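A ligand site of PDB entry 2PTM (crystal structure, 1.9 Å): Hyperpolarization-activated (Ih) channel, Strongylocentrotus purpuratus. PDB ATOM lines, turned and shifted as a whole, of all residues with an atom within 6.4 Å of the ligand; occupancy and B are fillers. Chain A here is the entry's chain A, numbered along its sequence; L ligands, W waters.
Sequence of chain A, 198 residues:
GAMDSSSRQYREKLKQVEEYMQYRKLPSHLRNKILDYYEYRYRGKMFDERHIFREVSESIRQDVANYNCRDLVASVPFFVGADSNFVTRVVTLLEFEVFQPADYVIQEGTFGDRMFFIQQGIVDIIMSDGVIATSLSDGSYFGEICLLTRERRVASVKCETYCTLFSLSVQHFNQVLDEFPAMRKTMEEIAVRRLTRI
Merely in contact with the ligand: Phe 142 (3.2 Å), Ala 155 (3.4 Å), Thr 134 (3.5 Å), Ile 125 (3.7 Å), Ile 106 (3.9 Å) and Val 157 (3.9 Å). Hydrophobic or aromatic side chains that line the ligand: Ile 106, Ile 125, Phe 142, Ile 145, Val 154, Ala 155 and Val 157. Within 4 Å of the ligand: Ile 106, Ile 125, Thr 134, Phe 142, Gly 143, Glu 144, Ile 145, Cys 146, Arg 153, Val 154, Ala 155, Val 157 and Arg 194.
Water W1 lies within hydrogen-bond range of N2 of the ligand (2.9 Å) and SD of Met 127 (3.7 Å).
The side-chain carboxylate (OE1) of Glu 144 is in hydrogen-bond range of an oxygen (O6) of the ligand (2.7 Å). An oxygen (O1) of the ligand lies within hydrogen-bond range of the backbone NH of Val 154, 2.8 Å away. N of Gly 143 is in hydrogen-bond range of O6 of the ligand (2.9 Å). NH1 of Arg 153 lies within salt-bridge range of O2 of the ligand (2.9 Å). The backbone NH (N) of Cys 146 sits at hydrogen-bond distance from an oxygen (O2) of the ligand (3.0 Å). The guanidinium group (NH1) of Arg 194 sits at hydrogen-bond distance from an oxygen (O6) of the ligand. The backbone NH (N) of Ile 145 lies close to an oxygen (O5) of the ligand (3.4 Å).
The side-chain carboxylate (OE2) of Glu 144 lies within salt-bridge range of the guanidinium group (NH1) of Arg 194 (3.1 Å). The backbone carbonyl oxygen (O) of Gly 143 is in hydrogen-bond range of the guanidinium group (NH1) of Arg 153 (2.8 Å). The guanidinium group (NH2) of Arg 153 sits at hydrogen-bond distance from the backbone carbonyl oxygen (O) of Arg 114 (2.8 Å). The side-chain sulfur (SG) of Cys 146 sits at hydrogen-bond distance from the backbone NH (N) of Gly 112, at 3.3 Å. The guanidinium group of Arg 194 sits at hydrogen-bond distance from the backbone carbonyl oxygen of Tyr 141 (2.9 Å). N of Ile 125 is in hydrogen-bond range of O of Thr 134 (2.8 Å). The backbone NH (N) of Ala 133 lies within hydrogen-bond range of the backbone carbonyl oxygen (O) of Ile 125. The backbone carbonyl oxygen (O) of Ile 106 sits at hydrogen-bond distance from the backbone NH (N) of Val 157 (2.9 Å).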
ATOM      1  N   ILE A 106      -8.054  -3.816  31.254  1.00  0.00           N
ATOM      2  CA  ILE A 106      -7.458  -3.066  30.141  1.00  0.00           C
ATOM      3  C   ILE A 106      -8.517  -2.736  29.120  1.00  0.00           C
ATOM      4  O   ILE A 106      -9.348  -3.585  28.797  1.00  0.00           O
ATOM      5  CB  ILE A 106      -6.351  -3.879  29.443  1.00  0.00           C
ATOM      6  CG1 ILE A 106      -5.109  -3.978  30.335  1.00  0.00           C
ATOM      7  CG2 ILE A 106      -5.956  -3.242  28.103  1.00  0.00           C
ATOM      8  CD1 ILE A 106      -3.979  -4.837  29.718  1.00  0.00           C
ATOM      9  N   GLY A 112      -0.981   2.415  28.072  1.00  0.00           N
ATOM     10  CA  GLY A 112      -0.775   1.454  29.141  1.00  0.00           C
ATOM     11  C   GLY A 112       0.352   1.886  30.067  1.00  0.00           C
ATOM     12  O   GLY A 112       1.361   2.426  29.619  1.00  0.00           O
ATOM     13  N   ARG A 114       1.355  -0.370  32.711  1.00  0.00           N
ATOM     14  CA  ARG A 114       1.879  -1.576  33.355  1.00  0.00           C
ATOM     15  C   ARG A 114       1.393  -2.835  32.626  1.00  0.00           C
ATOM     16  O   ARG A 114       0.446  -2.775  31.835  1.00  0.00           O
ATOM     17  CB  ARG A 114       1.474  -1.622  34.841  1.00  0.00           C
ATOM     18  CG  ARG A 114      -0.038  -1.756  35.105  1.00  0.00           C
ATOM     19  CD  ARG A 114      -0.380  -1.276  36.519  1.00  0.00           C
ATOM     20  NE  ARG A 114      -1.710  -1.680  36.980  1.00  0.00           N
ATOM     21  CZ  ARG A 114      -2.842  -1.058  36.652  1.00  0.00           C
ATOM     22  NH1 ARG A 114      -2.808   0.002  35.838  1.00  0.00           N
ATOM     23  NH2 ARG A 114      -4.001  -1.492  37.121  1.00  0.00           N
ATOM     24  N   ILE A 125      -9.771 -11.942  26.264  1.00  0.00           N
ATOM     25  CA  ILE A 125      -9.141 -10.957  25.394  1.00  0.00           C
ATOM     26  C   ILE A 125     -10.163 -10.566  24.326  1.00  0.00           C
ATOM     27  O   ILE A 125     -10.560 -11.396  23.515  1.00  0.00           O
ATOM     28  CB  ILE A 125      -7.871 -11.529  24.719  1.00  0.00           C
ATOM     29  CG1 ILE A 125      -6.907 -12.124  25.768  1.00  0.00           C
ATOM     30  CG2 ILE A 125      -7.186 -10.473  23.847  1.00  0.00           C
ATOM     31  CD1 ILE A 125      -6.508 -11.162  26.850  1.00  0.00           C
ATOM     32  N   MET A 127     -11.349  -8.215  21.160  1.00  0.00           N
ATOM     33  CA  MET A 127     -10.900  -7.335  20.085  1.00  0.00           C
ATOM     34  C   MET A 127     -11.806  -6.123  19.951  1.00  0.00           C
ATOM     35  O   MET A 127     -12.893  -6.083  20.521  1.00  0.00           O
ATOM     36  CB  MET A 127     -10.825  -8.106  18.756  1.00  0.00           C
ATOM     37  CG  MET A 127      -9.909  -9.312  18.806  1.00  0.00           C
ATOM     38  SD  MET A 127      -8.354  -8.957  19.662  1.00  0.00           S
ATOM     39  CE  MET A 127      -7.680  -7.641  18.629  1.00  0.00           C
ATOM     40  N   ALA A 133     -10.887 -13.078  21.318  1.00  0.00           N
ATOM     41  CA  ALA A 133      -9.799 -13.756  20.632  1.00  0.00           C
ATOM     42  C   ALA A 133      -9.445 -15.031  21.381  1.00  0.00           C
ATOM     43  O   ALA A 133      -9.219 -16.080  20.789  1.00  0.00           O
ATOM     44  CB  ALA A 133      -8.585 -12.846  20.519  1.00  0.00           C
ATOM     45  N   THR A 134      -9.402 -14.933  22.700  1.00  0.00           N
ATOM     46  CA  THR A 134      -8.998 -16.053  23.520  1.00  0.00           C
ATOM     47  C   THR A 134      -9.221 -15.693  24.976  1.00  0.00           C
ATOM     48  O   THR A 134      -9.567 -14.544  25.294  1.00  0.00           O
ATOM     49  CB  THR A 134      -7.509 -16.382  23.318  1.00  0.00           C
ATOM     50  OG1 THR A 134      -7.210 -17.660  23.891  1.00  0.00           O
ATOM     51  CG2 THR A 134      -6.633 -15.304  23.955  1.00  0.00           C
ATOM     52  N   LEU A 136      -7.311 -16.178  28.926  1.00  0.00           N
ATOM     53  CA  LEU A 136      -6.034 -16.469  29.573  1.00  0.00           C
ATOM     54  C   LEU A 136      -6.270 -16.789  31.032  1.00  0.00           C
ATOM     55  O   LEU A 136      -7.250 -16.324  31.618  1.00  0.00           O
ATOM     56  CB  LEU A 136      -5.090 -15.265  29.454  1.00  0.00           C
ATOM     57  CG  LEU A 136      -4.695 -14.783  28.066  1.00  0.00           C
ATOM     58  CD1 LEU A 136      -3.795 -13.558  28.192  1.00  0.00           C
ATOM     59  CD2 LEU A 136      -4.002 -15.888  27.279  1.00  0.00           C
ATOM     60  N   TYR A 141       0.192 -14.080  31.067  1.00  0.00           N
ATOM     61  CA  TYR A 141       0.391 -12.664  31.317  1.00  0.00           C
ATOM     62  C   TYR A 141      -0.202 -11.873  30.166  1.00  0.00           C
ATOM     63  O   TYR A 141      -0.457 -12.436  29.101  1.00  0.00           O
ATOM     64  CB  TYR A 141       1.862 -12.332  31.535  1.00  0.00           C
ATOM     65  CG  TYR A 141       2.782 -12.610  30.360  1.00  0.00           C
ATOM     66  CD1 TYR A 141       2.677 -11.889  29.182  1.00  0.00           C
ATOM     67  CD2 TYR A 141       3.775 -13.571  30.448  1.00  0.00           C
ATOM     68  CE1 TYR A 141       3.520 -12.127  28.104  1.00  0.00           C
ATOM     69  CE2 TYR A 141       4.635 -13.824  29.375  1.00  0.00           C
ATOM     70  CZ  TYR A 141       4.501 -13.094  28.219  1.00  0.00           C
ATOM     71  OH  TYR A 141       5.347 -13.342  27.163  1.00  0.00           O
ATOM     72  N   PHE A 142      -0.454 -10.590  30.392  1.00  0.00           N
ATOM     73  CA  PHE A 142      -1.034  -9.771  29.345  1.00  0.00           C
ATOM     74  C   PHE A 142      -0.730  -8.307  29.612  1.00  0.00           C
ATOM     75  O   PHE A 142      -0.342  -7.947  30.718  1.00  0.00           O
ATOM     76  CB  PHE A 142      -2.547  -9.981  29.249  1.00  0.00           C
ATOM     77  CG  PHE A 142      -3.291  -9.610  30.521  1.00  0.00           C
ATOM     78  CD1 PHE A 142      -3.663  -8.295  30.774  1.00  0.00           C
ATOM     79  CD2 PHE A 142      -3.629 -10.580  31.458  1.00  0.00           C
ATOM     80  CE1 PHE A 142      -4.351  -7.952  31.953  1.00  0.00           C
ATOM     81  CE2 PHE A 142      -4.309 -10.256  32.636  1.00  0.00           C
ATOM     82  CZ  PHE A 142      -4.672  -8.948  32.881  1.00  0.00           C
ATOM     83  N   GLY A 143      -0.906  -7.466  28.586  1.00  0.00           N
ATOM     84  CA  GLY A 143      -0.688  -6.040  28.711  1.00  0.00           C
ATOM     85  C   GLY A 143       0.753  -5.674  28.410  1.00  0.00           C
ATOM     86  O   GLY A 143       1.205  -4.560  28.701  1.00  0.00           O
ATOM     87  N   GLU A 144       1.483  -6.608  27.807  1.00  0.00           N
ATOM     88  CA  GLU A 144       2.885  -6.360  27.494  1.00  0.00           C
ATOM     89  C   GLU A 144       3.084  -5.661  26.140  1.00  0.00           C
ATOM     90  O   GLU A 144       4.079  -4.973  25.936  1.00  0.00           O
ATOM     91  CB  GLU A 144       3.686  -7.674  27.507  1.00  0.00           C
ATOM     92  CG  GLU A 144       3.564  -8.517  26.246  1.00  0.00           C
ATOM     93  CD  GLU A 144       2.255  -9.271  26.145  1.00  0.00           C
ATOM     94  OE1 GLU A 144       1.444  -9.215  27.081  1.00  0.00           O
ATOM     95  OE2 GLU A 144       2.034  -9.929  25.118  1.00  0.00           O
ATOM     96  N   ILE A 145       2.141  -5.840  25.215  1.00  0.00           N
ATOM     97  CA  ILE A 145       2.344  -5.371  23.843  1.00  0.00           C
ATOM     98  C   ILE A 145       2.565  -3.866  23.840  1.00  0.00           C
ATOM     99  O   ILE A 145       3.521  -3.360  23.255  1.00  0.00           O
ATOM    100  CB  ILE A 145       1.141  -5.682  22.908  1.00  0.00           C
ATOM    101  CG1 ILE A 145       0.849  -7.176  22.833  1.00  0.00           C
ATOM    102  CG2 ILE A 145       1.396  -5.123  21.526  1.00  0.00           C
ATOM    103  CD1 ILE A 145       2.041  -7.986  22.599  1.00  0.00           C
ATOM    104  N   CYS A 146       1.652  -3.160  24.505  1.00  0.00           N
ATOM    105  CA  CYS A 146       1.695  -1.706  24.607  1.00  0.00           C
ATOM    106  C   CYS A 146       3.018  -1.203  25.214  1.00  0.00           C
ATOM    107  O   CYS A 146       3.527  -0.157  24.834  1.00  0.00           O
ATOM    108  CB  CYS A 146       0.516  -1.248  25.470  1.00  0.00           C
ATOM    109  SG  CYS A 146       0.351   0.506  25.667  1.00  0.00           S
ATOM    110  N   LEU A 147       3.563  -1.960  26.167  1.00  0.00           N
ATOM    111  CA  LEU A 147       4.838  -1.590  26.787  1.00  0.00           C
ATOM    112  C   LEU A 147       6.012  -1.785  25.836  1.00  0.00           C
ATOM    113  O   LEU A 147       7.040  -1.107  25.941  1.00  0.00           O
ATOM    114  CB  LEU A 147       5.085  -2.411  28.057  1.00  0.00           C
ATOM    115  CG  LEU A 147       4.023  -2.320  29.153  1.00  0.00           C
ATOM    116  CD1 LEU A 147       4.564  -2.904  30.440  1.00  0.00           C
ATOM    117  CD2 LEU A 147       3.631  -0.882  29.368  1.00  0.00           C
ATOM    118  N   ARG A 152      -0.505   1.923  21.793  1.00  0.00           N
ATOM    119  CA  ARG A 152      -1.734   1.785  22.570  1.00  0.00           C
ATOM    120  C   ARG A 152      -2.105   0.330  22.785  1.00  0.00           C
ATOM    121  O   ARG A 152      -1.622  -0.543  22.086  1.00  0.00           O
ATOM    122  CB  ARG A 152      -2.891   2.519  21.881  1.00  0.00           C
ATOM    123  CG  ARG A 152      -2.610   3.999  21.651  1.00  0.00           C
ATOM    124  CD  ARG A 152      -3.704   4.642  20.824  1.00  0.00           C
ATOM    125  NE  ARG A 152      -3.477   6.073  20.659  1.00  0.00           N
ATOM    126  CZ  ARG A 152      -4.032   7.011  21.428  1.00  0.00           C
ATOM    127  NH1 ARG A 152      -4.863   6.649  22.404  1.00  0.00           N
ATOM    128  NH2 ARG A 152      -3.786   8.298  21.215  1.00  0.00           N
ATOM    129  N   ARG A 153      -2.991   0.085  23.762  1.00  0.00           N
ATOM    130  CA  ARG A 153      -3.536  -1.253  24.010  1.00  0.00           C
ATOM    131  C   ARG A 153      -4.210  -1.790  22.745  1.00  0.00           C
ATOM    132  O   ARG A 153      -4.992  -1.080  22.120  1.00  0.00           O
ATOM    133  CB  ARG A 153      -4.553  -1.196  25.141  1.00  0.00           C
ATOM    134  CG  ARG A 153      -4.019  -0.670  26.483  1.00  0.00           C
ATOM    135  CD  ARG A 153      -2.940  -1.550  27.076  1.00  0.00           C
ATOM    136  NE  ARG A 153      -2.751  -1.307  28.501  1.00  0.00           N
ATOM    137  CZ  ARG A 153      -1.819  -1.882  29.253  1.00  0.00           C
ATOM    138  NH1 ARG A 153      -0.969  -2.739  28.705  1.00  0.00           N
ATOM    139  NH2 ARG A 153      -1.746  -1.604  30.550  1.00  0.00           N
ATOM    140  N   VAL A 154      -3.951  -3.046  22.381  1.00  0.00           N
ATOM    141  CA  VAL A 154      -4.479  -3.581  21.121  1.00  0.00           C
ATOM    142  C   VAL A 154      -5.753  -4.398  21.283  1.00  0.00           C
ATOM    143  O   VAL A 154      -6.359  -4.818  20.295  1.00  0.00           O
ATOM    144  CB  VAL A 154      -3.414  -4.402  20.332  1.00  0.00           C
ATOM    145  CG1 VAL A 154      -2.148  -3.589  20.165  1.00  0.00           C
ATOM    146  CG2 VAL A 154      -3.130  -5.743  21.020  1.00  0.00           C
ATOM    147  N   ALA A 155      -6.169  -4.591  22.525  1.00  0.00           N
ATOM    148  CA  ALA A 155      -7.345  -5.397  22.829  1.00  0.00           C
ATOM    149  C   ALA A 155      -7.811  -4.974  24.203  1.00  0.00           C
ATOM    150  O   ALA A 155      -7.050  -4.347  24.939  1.00  0.00           O
ATOM    151  CB  ALA A 155      -6.982  -6.883  22.826  1.00  0.00           C
ATOM    152  N   SER A 156      -9.041  -5.308  24.569  1.00  0.00           N
ATOM    153  CA  SER A 156      -9.468  -5.132  25.961  1.00  0.00           C
ATOM    154  C   SER A 156      -9.276  -6.438  26.714  1.00  0.00           C
ATOM    155  O   SER A 156      -9.221  -7.512  26.111  1.00  0.00           O
ATOM    156  CB  SER A 156     -10.923  -4.675  26.028  1.00  0.00           C
ATOM    157  OG  SER A 156     -11.126  -3.484  25.300  1.00  0.00           O
ATOM    158  N   VAL A 157      -9.163  -6.363  28.038  1.00  0.00           N
ATOM    159  CA  VAL A 157      -9.045  -7.561  28.849  1.00  0.00           C
ATOM    160  C   VAL A 157     -10.066  -7.472  29.964  1.00  0.00           C
ATOM    161  O   VAL A 157     -10.043  -6.518  30.758  1.00  0.00           O
ATOM    162  CB  VAL A 157      -7.630  -7.688  29.454  1.00  0.00           C
ATOM    163  CG1 VAL A 157      -7.515  -8.976  30.299  1.00  0.00           C
ATOM    164  CG2 VAL A 157      -6.577  -7.662  28.325  1.00  0.00           C
ATOM    165  N   ARG A 193       3.643 -13.298  18.350  1.00  0.00           N
ATOM    166  CA  ARG A 193       2.803 -14.496  18.271  1.00  0.00           C
ATOM    167  C   ARG A 193       1.504 -14.325  19.030  1.00  0.00           C
ATOM    168  O   ARG A 193       0.934 -15.290  19.536  1.00  0.00           O
ATOM    169  CB  ARG A 193       3.501 -15.720  18.847  1.00  0.00           C
ATOM    170  CG  ARG A 193       4.698 -16.203  18.101  1.00  0.00           C
ATOM    171  CD  ARG A 193       4.824 -17.702  18.252  1.00  0.00           C
ATOM    172  NE  ARG A 193       6.034 -18.202  17.622  1.00  0.00           N
ATOM    173  CZ  ARG A 193       6.260 -19.474  17.307  1.00  0.00           C
ATOM    174  NH1 ARG A 193       5.340 -20.392  17.562  1.00  0.00           N
ATOM    175  NH2 ARG A 193       7.405 -19.829  16.737  1.00  0.00           N
ATOM    176  N   ARG A 194       1.056 -13.078  19.151  1.00  0.00           N
ATOM    177  CA  ARG A 194      -0.311 -12.792  19.517  1.00  0.00           C
ATOM    178  C   ARG A 194      -0.794 -12.059  18.270  1.00  0.00           C
ATOM    179  O   ARG A 194      -0.836 -10.831  18.209  1.00  0.00           O
ATOM    180  CB  ARG A 194      -0.369 -12.024  20.842  1.00  0.00           C
ATOM    181  CG  ARG A 194      -0.174 -13.012  22.035  1.00  0.00           C
ATOM    182  CD  ARG A 194       0.116 -12.391  23.417  1.00  0.00           C
ATOM    183  NE  ARG A 194      -0.048 -13.435  24.455  1.00  0.00           N
ATOM    184  CZ  ARG A 194      -0.093 -13.223  25.770  1.00  0.00           C
ATOM    185  NH1 ARG A 194       0.029 -12.000  26.255  1.00  0.00           N
ATOM    186  NH2 ARG A 194      -0.268 -14.239  26.617  1.00  0.00           N
ATOM    187  N   LEU A 195      -1.112 -12.885  17.282  1.00  0.00           N
ATOM    188  CA  LEU A 195      -1.011 -12.573  15.846  1.00  0.00           C
ATOM    189  C   LEU A 195      -1.622 -11.276  15.318  1.00  0.00           C
ATOM    190  O   LEU A 195      -2.178 -10.448  16.049  1.00  0.00           O
ATOM    191  CB  LEU A 195      -1.483 -13.781  15.033  1.00  0.00           C
ATOM    192  CG  LEU A 195      -0.682 -15.053  15.307  1.00  0.00           C
ATOM    193  CD1 LEU A 195      -1.366 -16.295  14.748  1.00  0.00           C
ATOM    194  CD2 LEU A 195       0.748 -14.922  14.786  1.00  0.00           C
HETATM  195  P1  LIG L   1      -1.714  -4.805  25.325  1.00  0.00           P
HETATM  196  O1  LIG L   1      -2.016  -4.328  23.868  1.00  0.00           O
HETATM  197  O2  LIG L   1      -0.735  -4.067  26.093  1.00  0.00           O
HETATM  198  O3  LIG L   1      -3.213  -4.892  25.926  1.00  0.00           O
HETATM  199  C1  LIG L   1      -4.113  -5.951  25.736  1.00  0.00           C
HETATM  200  C2  LIG L   1      -3.467  -7.317  25.878  1.00  0.00           C
HETATM  201  O4  LIG L   1      -4.189  -8.423  25.343  1.00  0.00           O
HETATM  202  C3  LIG L   1      -2.237  -7.320  24.999  1.00  0.00           C
HETATM  203  O5  LIG L   1      -1.256  -6.345  25.141  1.00  0.00           O
HETATM  204  C4  LIG L   1      -1.747  -8.769  24.965  1.00  0.00           C
HETATM  205  O6  LIG L   1      -1.165  -9.081  26.223  1.00  0.00           O
HETATM  206  C5  LIG L   1      -3.171  -9.424  25.001  1.00  0.00           C
HETATM  207  N1  LIG L   1      -3.526  -9.999  23.736  1.00  0.00           N
HETATM  208  C6  LIG L   1      -3.911  -9.353  22.539  1.00  0.00           C
HETATM  209  N2  LIG L   1      -4.229 -10.223  21.563  1.00  0.00           N
HETATM  210  C7  LIG L   1      -4.016 -11.485  22.121  1.00  0.00           C
HETATM  211  C8  LIG L   1      -4.136 -12.829  21.642  1.00  0.00           C
HETATM  212  N3  LIG L   1      -4.558 -13.071  20.354  1.00  0.00           N
HETATM  213  N4  LIG L   1      -3.829 -13.862  22.471  1.00  0.00           N
HETATM  214  C9  LIG L   1      -3.436 -13.589  23.740  1.00  0.00           C
HETATM  215  N5  LIG L   1      -3.280 -12.394  24.337  1.00  0.00           N
HETATM  216  C10 LIG L   1      -3.592 -11.375  23.504  1.00  0.00           C
HETATM  217  O   HOH W   1      -4.809  -9.270  18.842  1.00  0.00           O
HETATM  218  O   HOH W   2      -4.442 -15.675  18.612  1.00  0.00           O
HETATM  219  O   HOH W   3      -3.513 -16.359  21.842  1.00  0.00           O
